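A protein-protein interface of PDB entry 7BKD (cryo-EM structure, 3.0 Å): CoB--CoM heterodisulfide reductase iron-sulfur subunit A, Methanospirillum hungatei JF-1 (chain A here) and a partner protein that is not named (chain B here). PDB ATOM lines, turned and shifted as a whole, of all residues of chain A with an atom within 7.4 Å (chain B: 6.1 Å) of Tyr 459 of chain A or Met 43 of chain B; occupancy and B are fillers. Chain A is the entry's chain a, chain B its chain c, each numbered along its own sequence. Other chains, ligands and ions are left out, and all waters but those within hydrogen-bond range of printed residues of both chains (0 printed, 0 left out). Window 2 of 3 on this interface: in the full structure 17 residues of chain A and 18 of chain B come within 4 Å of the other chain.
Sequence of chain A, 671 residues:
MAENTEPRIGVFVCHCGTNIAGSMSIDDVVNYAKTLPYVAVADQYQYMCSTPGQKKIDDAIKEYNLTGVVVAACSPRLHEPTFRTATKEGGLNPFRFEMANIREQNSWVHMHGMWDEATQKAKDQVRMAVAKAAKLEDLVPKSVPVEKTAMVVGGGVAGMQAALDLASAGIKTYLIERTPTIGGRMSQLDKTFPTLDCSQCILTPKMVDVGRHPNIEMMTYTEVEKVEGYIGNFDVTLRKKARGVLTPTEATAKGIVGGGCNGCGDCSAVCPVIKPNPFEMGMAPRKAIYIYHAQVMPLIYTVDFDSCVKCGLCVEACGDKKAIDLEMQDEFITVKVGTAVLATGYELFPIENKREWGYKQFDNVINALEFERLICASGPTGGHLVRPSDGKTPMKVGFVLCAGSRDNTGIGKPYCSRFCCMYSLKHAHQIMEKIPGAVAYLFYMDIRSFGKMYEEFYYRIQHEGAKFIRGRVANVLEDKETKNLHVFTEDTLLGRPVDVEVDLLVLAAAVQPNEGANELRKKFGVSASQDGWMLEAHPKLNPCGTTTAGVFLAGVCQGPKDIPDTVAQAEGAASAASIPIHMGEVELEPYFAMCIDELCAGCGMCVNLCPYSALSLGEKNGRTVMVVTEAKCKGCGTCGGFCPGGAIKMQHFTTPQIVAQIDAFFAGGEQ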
ATOM      1  N   LEU A 425      11.897 -19.163 -10.382  1.00  0.00           N
ATOM      2  CA  LEU A 425      10.748 -18.811 -11.211  1.00  0.00           C
ATOM      3  C   LEU A 425      10.743 -19.607 -12.511  1.00  0.00           C
ATOM      4  O   LEU A 425       9.689 -20.072 -12.964  1.00  0.00           O
ATOM      5  CB  LEU A 425      10.753 -17.313 -11.509  1.00  0.00           C
ATOM      6  CG  LEU A 425      10.479 -16.354 -10.353  1.00  0.00           C
ATOM      7  CD1 LEU A 425      10.865 -14.939 -10.735  1.00  0.00           C
ATOM      8  CD2 LEU A 425       9.026 -16.418  -9.945  1.00  0.00           C
ATOM      9  N   SER A 449      13.864  -9.775  -8.761  1.00  0.00           N
ATOM     10  CA  SER A 449      13.882  -9.747 -10.221  1.00  0.00           C
ATOM     11  C   SER A 449      14.241  -8.318 -10.616  1.00  0.00           C
ATOM     12  O   SER A 449      13.366  -7.490 -10.876  1.00  0.00           O
ATOM     13  CB  SER A 449      12.540 -10.185 -10.804  1.00  0.00           C
ATOM     14  OG  SER A 449      11.469  -9.445 -10.247  1.00  0.00           O
ATOM     15  N   TYR A 454      13.276  -8.989 -16.059  1.00  0.00           N
ATOM     16  CA  TYR A 454      13.178  -9.898 -14.923  1.00  0.00           C
ATOM     17  C   TYR A 454      11.846  -9.736 -14.200  1.00  0.00           C
ATOM     18  O   TYR A 454      11.234 -10.726 -13.787  1.00  0.00           O
ATOM     19  CB  TYR A 454      14.359  -9.638 -13.986  1.00  0.00           C
ATOM     20  CG  TYR A 454      15.687 -10.173 -14.491  1.00  0.00           C
ATOM     21  CD1 TYR A 454      16.364 -11.167 -13.808  1.00  0.00           C
ATOM     22  CD2 TYR A 454      16.193  -9.776 -15.715  1.00  0.00           C
ATOM     23  CE1 TYR A 454      17.557 -11.672 -14.276  1.00  0.00           C
ATOM     24  CE2 TYR A 454      17.378 -10.279 -16.198  1.00  0.00           C
ATOM     25  CZ  TYR A 454      18.056 -11.230 -15.477  1.00  0.00           C
ATOM     26  OH  TYR A 454      19.240 -11.736 -15.960  1.00  0.00           O
ATOM     27  N   GLU A 455      11.382  -8.496 -14.045  1.00  0.00           N
ATOM     28  CA  GLU A 455      10.110  -8.260 -13.371  1.00  0.00           C
ATOM     29  C   GLU A 455       8.940  -8.757 -14.212  1.00  0.00           C
ATOM     30  O   GLU A 455       7.966  -9.296 -13.674  1.00  0.00           O
ATOM     31  CB  GLU A 455       9.960  -6.775 -13.045  1.00  0.00           C
ATOM     32  CG  GLU A 455       8.687  -6.421 -12.303  1.00  0.00           C
ATOM     33  CD  GLU A 455       8.825  -6.593 -10.799  1.00  0.00           C
ATOM     34  OE1 GLU A 455       7.792  -6.590 -10.098  1.00  0.00           O
ATOM     35  OE2 GLU A 455       9.968  -6.732 -10.319  1.00  0.00           O
ATOM     36  N   GLU A 456       9.018  -8.586 -15.532  1.00  0.00           N
ATOM     37  CA  GLU A 456       7.977  -9.110 -16.411  1.00  0.00           C
ATOM     38  C   GLU A 456       7.936 -10.632 -16.385  1.00  0.00           C
ATOM     39  O   GLU A 456       6.858 -11.224 -16.500  1.00  0.00           O
ATOM     40  CB  GLU A 456       8.190  -8.597 -17.835  1.00  0.00           C
ATOM     41  CG  GLU A 456       8.036  -7.089 -17.987  1.00  0.00           C
ATOM     42  CD  GLU A 456       9.260  -6.301 -17.545  1.00  0.00           C
ATOM     43  OE1 GLU A 456      10.176  -6.890 -16.933  1.00  0.00           O
ATOM     44  OE2 GLU A 456       9.306  -5.083 -17.816  1.00  0.00           O
ATOM     45  N   PHE A 457       9.091 -11.279 -16.229  1.00  0.00           N
ATOM     46  CA  PHE A 457       9.110 -12.722 -16.024  1.00  0.00           C
ATOM     47  C   PHE A 457       8.373 -13.095 -14.745  1.00  0.00           C
ATOM     48  O   PHE A 457       7.624 -14.076 -14.712  1.00  0.00           O
ATOM     49  CB  PHE A 457      10.555 -13.216 -15.985  1.00  0.00           C
ATOM     50  CG  PHE A 457      10.694 -14.704 -16.074  1.00  0.00           C
ATOM     51  CD1 PHE A 457      10.368 -15.376 -17.237  1.00  0.00           C
ATOM     52  CD2 PHE A 457      11.170 -15.431 -14.998  1.00  0.00           C
ATOM     53  CE1 PHE A 457      10.502 -16.743 -17.318  1.00  0.00           C
ATOM     54  CE2 PHE A 457      11.310 -16.796 -15.075  1.00  0.00           C
ATOM     55  CZ  PHE A 457      10.975 -17.455 -16.236  1.00  0.00           C
ATOM     56  N   TYR A 458       8.573 -12.312 -13.684  1.00  0.00           N
ATOM     57  CA  TYR A 458       7.864 -12.523 -12.426  1.00  0.00           C
ATOM     58  C   TYR A 458       6.356 -12.376 -12.612  1.00  0.00           C
ATOM     59  O   TYR A 458       5.571 -13.182 -12.094  1.00  0.00           O
ATOM     60  CB  TYR A 458       8.408 -11.527 -11.401  1.00  0.00           C
ATOM     61  CG  TYR A 458       7.758 -11.512 -10.043  1.00  0.00           C
ATOM     62  CD1 TYR A 458       7.316 -12.678  -9.440  1.00  0.00           C
ATOM     63  CD2 TYR A 458       7.620 -10.320  -9.347  1.00  0.00           C
ATOM     64  CE1 TYR A 458       6.735 -12.652  -8.192  1.00  0.00           C
ATOM     65  CE2 TYR A 458       7.044 -10.285  -8.101  1.00  0.00           C
ATOM     66  CZ  TYR A 458       6.602 -11.453  -7.527  1.00  0.00           C
ATOM     67  OH  TYR A 458       6.024 -11.416  -6.282  1.00  0.00           O
ATOM     68  N   TYR A 459       5.941 -11.357 -13.366  1.00  0.00           N
ATOM     69  CA  TYR A 459       4.528 -11.164 -13.676  1.00  0.00           C
ATOM     70  C   TYR A 459       3.960 -12.360 -14.429  1.00  0.00           C
ATOM     71  O   TYR A 459       2.873 -12.852 -14.106  1.00  0.00           O
ATOM     72  CB  TYR A 459       4.361  -9.877 -14.486  1.00  0.00           C
ATOM     73  CG  TYR A 459       2.963  -9.313 -14.512  1.00  0.00           C
ATOM     74  CD1 TYR A 459       2.006  -9.825 -15.376  1.00  0.00           C
ATOM     75  CD2 TYR A 459       2.598  -8.270 -13.675  1.00  0.00           C
ATOM     76  CE1 TYR A 459       0.730  -9.311 -15.406  1.00  0.00           C
ATOM     77  CE2 TYR A 459       1.325  -7.751 -13.699  1.00  0.00           C
ATOM     78  CZ  TYR A 459       0.394  -8.275 -14.565  1.00  0.00           C
ATOM     79  OH  TYR A 459      -0.880  -7.763 -14.593  1.00  0.00           O
ATOM     80  N   ARG A 460       4.691 -12.848 -15.434  1.00  0.00           N
ATOM     81  CA  ARG A 460       4.232 -14.014 -16.183  1.00  0.00           C
ATOM     82  C   ARG A 460       4.109 -15.238 -15.287  1.00  0.00           C
ATOM     83  O   ARG A 460       3.142 -16.001 -15.399  1.00  0.00           O
ATOM     84  CB  ARG A 460       5.179 -14.312 -17.343  1.00  0.00           C
ATOM     85  CG  ARG A 460       5.234 -13.254 -18.421  1.00  0.00           C
ATOM     86  CD  ARG A 460       6.222 -13.661 -19.502  1.00  0.00           C
ATOM     87  NE  ARG A 460       5.765 -14.846 -20.222  1.00  0.00           N
ATOM     88  CZ  ARG A 460       6.329 -16.046 -20.121  1.00  0.00           C
ATOM     89  NH1 ARG A 460       7.378 -16.223 -19.332  1.00  0.00           N
ATOM     90  NH2 ARG A 460       5.847 -17.070 -20.812  1.00  0.00           N
ATOM     91  N   ILE A 461       5.088 -15.456 -14.408  1.00  0.00           N
ATOM     92  CA  ILE A 461       5.057 -16.638 -13.554  1.00  0.00           C
ATOM     93  C   ILE A 461       3.863 -16.580 -12.613  1.00  0.00           C
ATOM     94  O   ILE A 461       3.166 -17.583 -12.411  1.00  0.00           O
ATOM     95  CB  ILE A 461       6.380 -16.793 -12.781  1.00  0.00           C
ATOM     96  CG1 ILE A 461       7.554 -16.977 -13.743  1.00  0.00           C
ATOM     97  CG2 ILE A 461       6.309 -17.987 -11.849  1.00  0.00           C
ATOM     98  CD1 ILE A 461       7.238 -17.819 -14.952  1.00  0.00           C
ATOM     99  N   GLN A 462       3.604 -15.411 -12.024  1.00  0.00           N
ATOM    100  CA  GLN A 462       2.424 -15.286 -11.175  1.00  0.00           C
ATOM    101  C   GLN A 462       1.144 -15.491 -11.977  1.00  0.00           C
ATOM    102  O   GLN A 462       0.192 -16.114 -11.492  1.00  0.00           O
ATOM    103  CB  GLN A 462       2.404 -13.931 -10.470  1.00  0.00           C
ATOM    104  CG  GLN A 462       1.257 -13.796  -9.482  1.00  0.00           C
ATOM    105  CD  GLN A 462       1.454 -12.673  -8.489  1.00  0.00           C
ATOM    106  OE1 GLN A 462       2.502 -12.032  -8.457  1.00  0.00           O
ATOM    107  NE2 GLN A 462       0.443 -12.431  -7.667  1.00  0.00           N
ATOM    108  N   HIS A 463       1.106 -14.984 -13.213  1.00  0.00           N
ATOM    109  CA  HIS A 463      -0.073 -15.160 -14.055  1.00  0.00           C
ATOM    110  C   HIS A 463      -0.327 -16.624 -14.389  1.00  0.00           C
ATOM    111  O   HIS A 463      -1.486 -17.040 -14.491  1.00  0.00           O
ATOM    112  CB  HIS A 463       0.077 -14.349 -15.341  1.00  0.00           C
ATOM    113  CG  HIS A 463      -1.210 -14.129 -16.068  1.00  0.00           C
ATOM    114  ND1 HIS A 463      -1.468 -14.682 -17.304  1.00  0.00           N
ATOM    115  CD2 HIS A 463      -2.318 -13.425 -15.733  1.00  0.00           C
ATOM    116  CE1 HIS A 463      -2.676 -14.324 -17.701  1.00  0.00           C
ATOM    117  NE2 HIS A 463      -3.213 -13.562 -16.765  1.00  0.00           N
ATOM    118  N   GLU A 464       0.728 -17.415 -14.574  1.00  0.00           N
ATOM    119  CA  GLU A 464       0.547 -18.821 -14.912  1.00  0.00           C
ATOM    120  C   GLU A 464       0.031 -19.652 -13.745  1.00  0.00           C
ATOM    121  O   GLU A 464      -0.357 -20.805 -13.956  1.00  0.00           O
ATOM    122  CB  GLU A 464       1.859 -19.414 -15.429  1.00  0.00           C
ATOM    123  CG  GLU A 464       2.350 -18.865 -16.773  1.00  0.00           C
ATOM    124  CD  GLU A 464       1.247 -18.561 -17.780  1.00  0.00           C
ATOM    125  OE1 GLU A 464       0.245 -19.307 -17.852  1.00  0.00           O
ATOM    126  OE2 GLU A 464       1.389 -17.560 -18.514  1.00  0.00           O
ATOM    127  N   GLY A 465       0.028 -19.111 -12.530  1.00  0.00           N
ATOM    128  CA  GLY A 465      -0.598 -19.792 -11.415  1.00  0.00           C
ATOM    129  C   GLY A 465       0.335 -20.195 -10.296  1.00  0.00           C
ATOM    130  O   GLY A 465      -0.045 -20.986  -9.428  1.00  0.00           O
ATOM    131  N   PHE A 468       2.880 -17.865  -4.255  1.00  0.00           N
ATOM    132  CA  PHE A 468       4.003 -17.224  -3.583  1.00  0.00           C
ATOM    133  C   PHE A 468       3.665 -17.063  -2.109  1.00  0.00           C
ATOM    134  O   PHE A 468       2.836 -16.225  -1.745  1.00  0.00           O
ATOM    135  CB  PHE A 468       4.333 -15.873  -4.215  1.00  0.00           C
ATOM    136  CG  PHE A 468       4.937 -15.975  -5.582  1.00  0.00           C
ATOM    137  CD1 PHE A 468       4.166 -16.360  -6.666  1.00  0.00           C
ATOM    138  CD2 PHE A 468       6.282 -15.721  -5.779  1.00  0.00           C
ATOM    139  CE1 PHE A 468       4.715 -16.458  -7.923  1.00  0.00           C
ATOM    140  CE2 PHE A 468       6.841 -15.827  -7.034  1.00  0.00           C
ATOM    141  CZ  PHE A 468       6.054 -16.196  -8.109  1.00  0.00           C
ATOM    142  N   ILE B  40      -8.352  -8.694 -12.330  1.00  0.00           N
ATOM    143  CA  ILE B  40      -7.201  -9.616 -12.264  1.00  0.00           C
ATOM    144  C   ILE B  40      -6.804  -9.700 -10.794  1.00  0.00           C
ATOM    145  O   ILE B  40      -5.841  -9.088 -10.328  1.00  0.00           O
ATOM    146  CB  ILE B  40      -6.045  -9.172 -13.170  1.00  0.00           C
ATOM    147  CG1 ILE B  40      -5.808  -7.664 -13.053  1.00  0.00           C
ATOM    148  CG2 ILE B  40      -6.317  -9.556 -14.609  1.00  0.00           C
ATOM    149  CD1 ILE B  40      -4.503  -7.204 -13.654  1.00  0.00           C
ATOM    150  N   ALA B  41      -7.548 -10.518 -10.050  1.00  0.00           N
ATOM    151  CA  ALA B  41      -7.344 -10.617  -8.610  1.00  0.00           C
ATOM    152  C   ALA B  41      -6.138 -11.471  -8.255  1.00  0.00           C
ATOM    153  O   ALA B  41      -5.478 -11.213  -7.244  1.00  0.00           O
ATOM    154  CB  ALA B  41      -8.599 -11.177  -7.943  1.00  0.00           C
ATOM    155  N   ASN B  42      -5.832 -12.479  -9.070  1.00  0.00           N
ATOM    156  CA  ASN B  42      -4.715 -13.371  -8.795  1.00  0.00           C
ATOM    157  C   ASN B  42      -3.364 -12.682  -8.919  1.00  0.00           C
ATOM    158  O   ASN B  42      -2.356 -13.268  -8.515  1.00  0.00           O
ATOM    159  CB  ASN B  42      -4.756 -14.561  -9.746  1.00  0.00           C
ATOM    160  CG  ASN B  42      -4.973 -14.142 -11.182  1.00  0.00           C
ATOM    161  OD1 ASN B  42      -5.978 -13.522 -11.513  1.00  0.00           O
ATOM    162  ND2 ASN B  42      -4.023 -14.481 -12.046  1.00  0.00           N
ATOM    163  N   MET B  43      -3.317 -11.471  -9.461  1.00  0.00           N
ATOM    164  CA  MET B  43      -2.067 -10.770  -9.706  1.00  0.00           C
ATOM    165  C   MET B  43      -1.624  -9.907  -8.536  1.00  0.00           C
ATOM    166  O   MET B  43      -0.639  -9.177  -8.662  1.00  0.00           O
ATOM    167  CB  MET B  43      -2.180  -9.909 -10.965  1.00  0.00           C
ATOM    168  CG  MET B  43      -2.248 -10.717 -12.239  1.00  0.00           C
ATOM    169  SD  MET B  43      -1.029 -12.046 -12.237  1.00  0.00           S
ATOM    170  CE  MET B  43       0.493 -11.121 -12.402  1.00  0.00           C
ATOM    171  N   CYS B  44      -2.332  -9.957  -7.413  1.00  0.00           N
ATOM    172  CA  CYS B  44      -1.922  -9.196  -6.245  1.00  0.00           C
ATOM    173  C   CYS B  44      -0.606  -9.733  -5.698  1.00  0.00           C
ATOM    174  O   CYS B  44      -0.414 -10.945  -5.581  1.00  0.00           O
ATOM    175  CB  CYS B  44      -3.011  -9.255  -5.173  1.00  0.00           C
ATOM    176  SG  CYS B  44      -2.590  -8.523  -3.588  1.00  0.00           S
ATOM    177  N   TYR B  45       0.314  -8.826  -5.374  1.00  0.00           N
ATOM    178  CA  TYR B  45       1.537  -9.211  -4.681  1.00  0.00           C
ATOM    179  C   TYR B  45       1.680  -8.504  -3.338  1.00  0.00           C
ATOM    180  O   TYR B  45       2.796  -8.352  -2.836  1.00  0.00           O
ATOM    181  CB  TYR B  45       2.770  -8.988  -5.563  1.00  0.00           C
ATOM    182  CG  TYR B  45       3.043  -7.565  -5.968  1.00  0.00           C
ATOM    183  CD1 TYR B  45       2.507  -7.046  -7.123  1.00  0.00           C
ATOM    184  CD2 TYR B  45       3.855  -6.747  -5.209  1.00  0.00           C
ATOM    185  CE1 TYR B  45       2.763  -5.753  -7.513  1.00  0.00           C
ATOM    186  CE2 TYR B  45       4.109  -5.451  -5.592  1.00  0.00           C
ATOM    187  CZ  TYR B  45       3.556  -4.956  -6.744  1.00  0.00           C
ATOM    188  OH  TYR B  45       3.804  -3.661  -7.136  1.00  0.00           O
ATOM    189  N   VAL B  72      -6.800 -15.088  -3.441  1.00  0.00           N
ATOM    190  CA  VAL B  72      -5.718 -15.742  -4.176  1.00  0.00           C
ATOM    191  C   VAL B  72      -5.524 -17.173  -3.692  1.00  0.00           C
ATOM    192  O   VAL B  72      -5.354 -18.098  -4.496  1.00  0.00           O
ATOM    193  CB  VAL B  72      -4.419 -14.921  -4.065  1.00  0.00           C
ATOM    194  CG1 VAL B  72      -3.270 -15.652  -4.731  1.00  0.00           C
ATOM    195  CG2 VAL B  72      -4.608 -13.567  -4.714  1.00  0.00           C
ATOM    196  N   ARG B 100      -1.220  -2.769  -9.504  1.00  0.00           N
ATOM    197  CA  ARG B 100      -1.400  -3.917 -10.378  1.00  0.00           C
ATOM    198  C   ARG B 100      -2.668  -3.833 -11.216  1.00  0.00           C
ATOM    199  O   ARG B 100      -3.020  -4.813 -11.877  1.00  0.00           O
ATOM    200  CB  ARG B 100      -1.410  -5.199  -9.546  1.00  0.00           C
ATOM    201  CG  ARG B 100      -0.043  -5.809  -9.333  1.00  0.00           C
ATOM    202  CD  ARG B 100       0.413  -6.576 -10.552  1.00  0.00           C
ATOM    203  NE  ARG B 100       1.847  -6.846 -10.529  1.00  0.00           N
ATOM    204  CZ  ARG B 100       2.388  -7.995 -10.145  1.00  0.00           C
ATOM    205  NH1 ARG B 100       1.621  -8.991  -9.730  1.00  0.00           N
ATOM    206  NH2 ARG B 100       3.703  -8.141 -10.161  1.00  0.00           N
ATOM    207  N   ILE B 102      -5.716  -3.787 -10.086  1.00  0.00           N
ATOM    208  CA  ILE B 102      -6.730  -4.628  -9.472  1.00  0.00           C
ATOM    209  C   ILE B 102      -7.810  -3.717  -8.915  1.00  0.00           C
ATOM    210  O   ILE B 102      -7.545  -2.587  -8.492  1.00  0.00           O
ATOM    211  CB  ILE B 102      -6.127  -5.529  -8.377  1.00  0.00           C
ATOM    212  CG1 ILE B 102      -4.936  -6.301  -8.936  1.00  0.00           C
ATOM    213  CG2 ILE B 102      -7.173  -6.480  -7.811  1.00  0.00           C
ATOM    214  CD1 ILE B 102      -4.247  -7.150  -7.923  1.00  0.00           C
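O of Asn 42 of chain B is in hydrogen-bond range of NE2 of Gln 462 of chain A (3.0 Å).
The side-chain amide nitrogen of Gln 462 of chain A sits at hydrogen-bond distance from the backbone carbonyl oxygen of Cys 44 of chain B, at 2.7 Å.
OE1 of Gln 462 of chain A lies within hydrogen-bond range of NH1 of Arg 100 of chain B (3.4 Å).
N of His 463 of chain A sits close to SD of Met 43 of chain B (3.8 Å).
The guanidinium group (NH1) of Arg 100 of chain B lies within hydrogen-bond range of the backbone carbonyl oxygen (O) of Met 43 of chain B (2.5 Å).
Among the printed residues, pairs that only touch across the chains: Tyr 459 of chain A with Arg 100 of chain B, Gln 462 of chain A with Met 43 of chain B, Tyr 459 of chain A with Met 43 of chain B and Tyr 459 of chain A with Ile 40 of chain B.
Of chain B, only Ile 40 (3.8 Å), Met 43 (3.4 Å) and Arg 100 (3.3 Å) come within 4 Å of Tyr 459 of chain A.
Met 43 of chain B touches three residues of chain A.
Printed residues of chain A within 4 Å of Cys 44 of chain B: Gln 462.
Printed residues of chain A within 4 Å of Asn 42 of chain B: Gln 462.
The nearest printed residue of chain B that does not touch Tyr 459 of chain A is Tyr 45 of chain B (6.7 Å).
The nearest residue of chain A that does not touch Met 43 of chain B is Arg 460 of chain A (5.5 Å).
Hydrophobic or aromatic side chains of chain B within 4 Å of the printed part of chain A: Ile 40 and Met 43.
Among the printed residues, 8 pairs touch across the chains.
Among the printed residues, no Asp or Glu carboxylate lies within 4 Å of a Lys or Arg side-chain nitrogen of the other chain.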
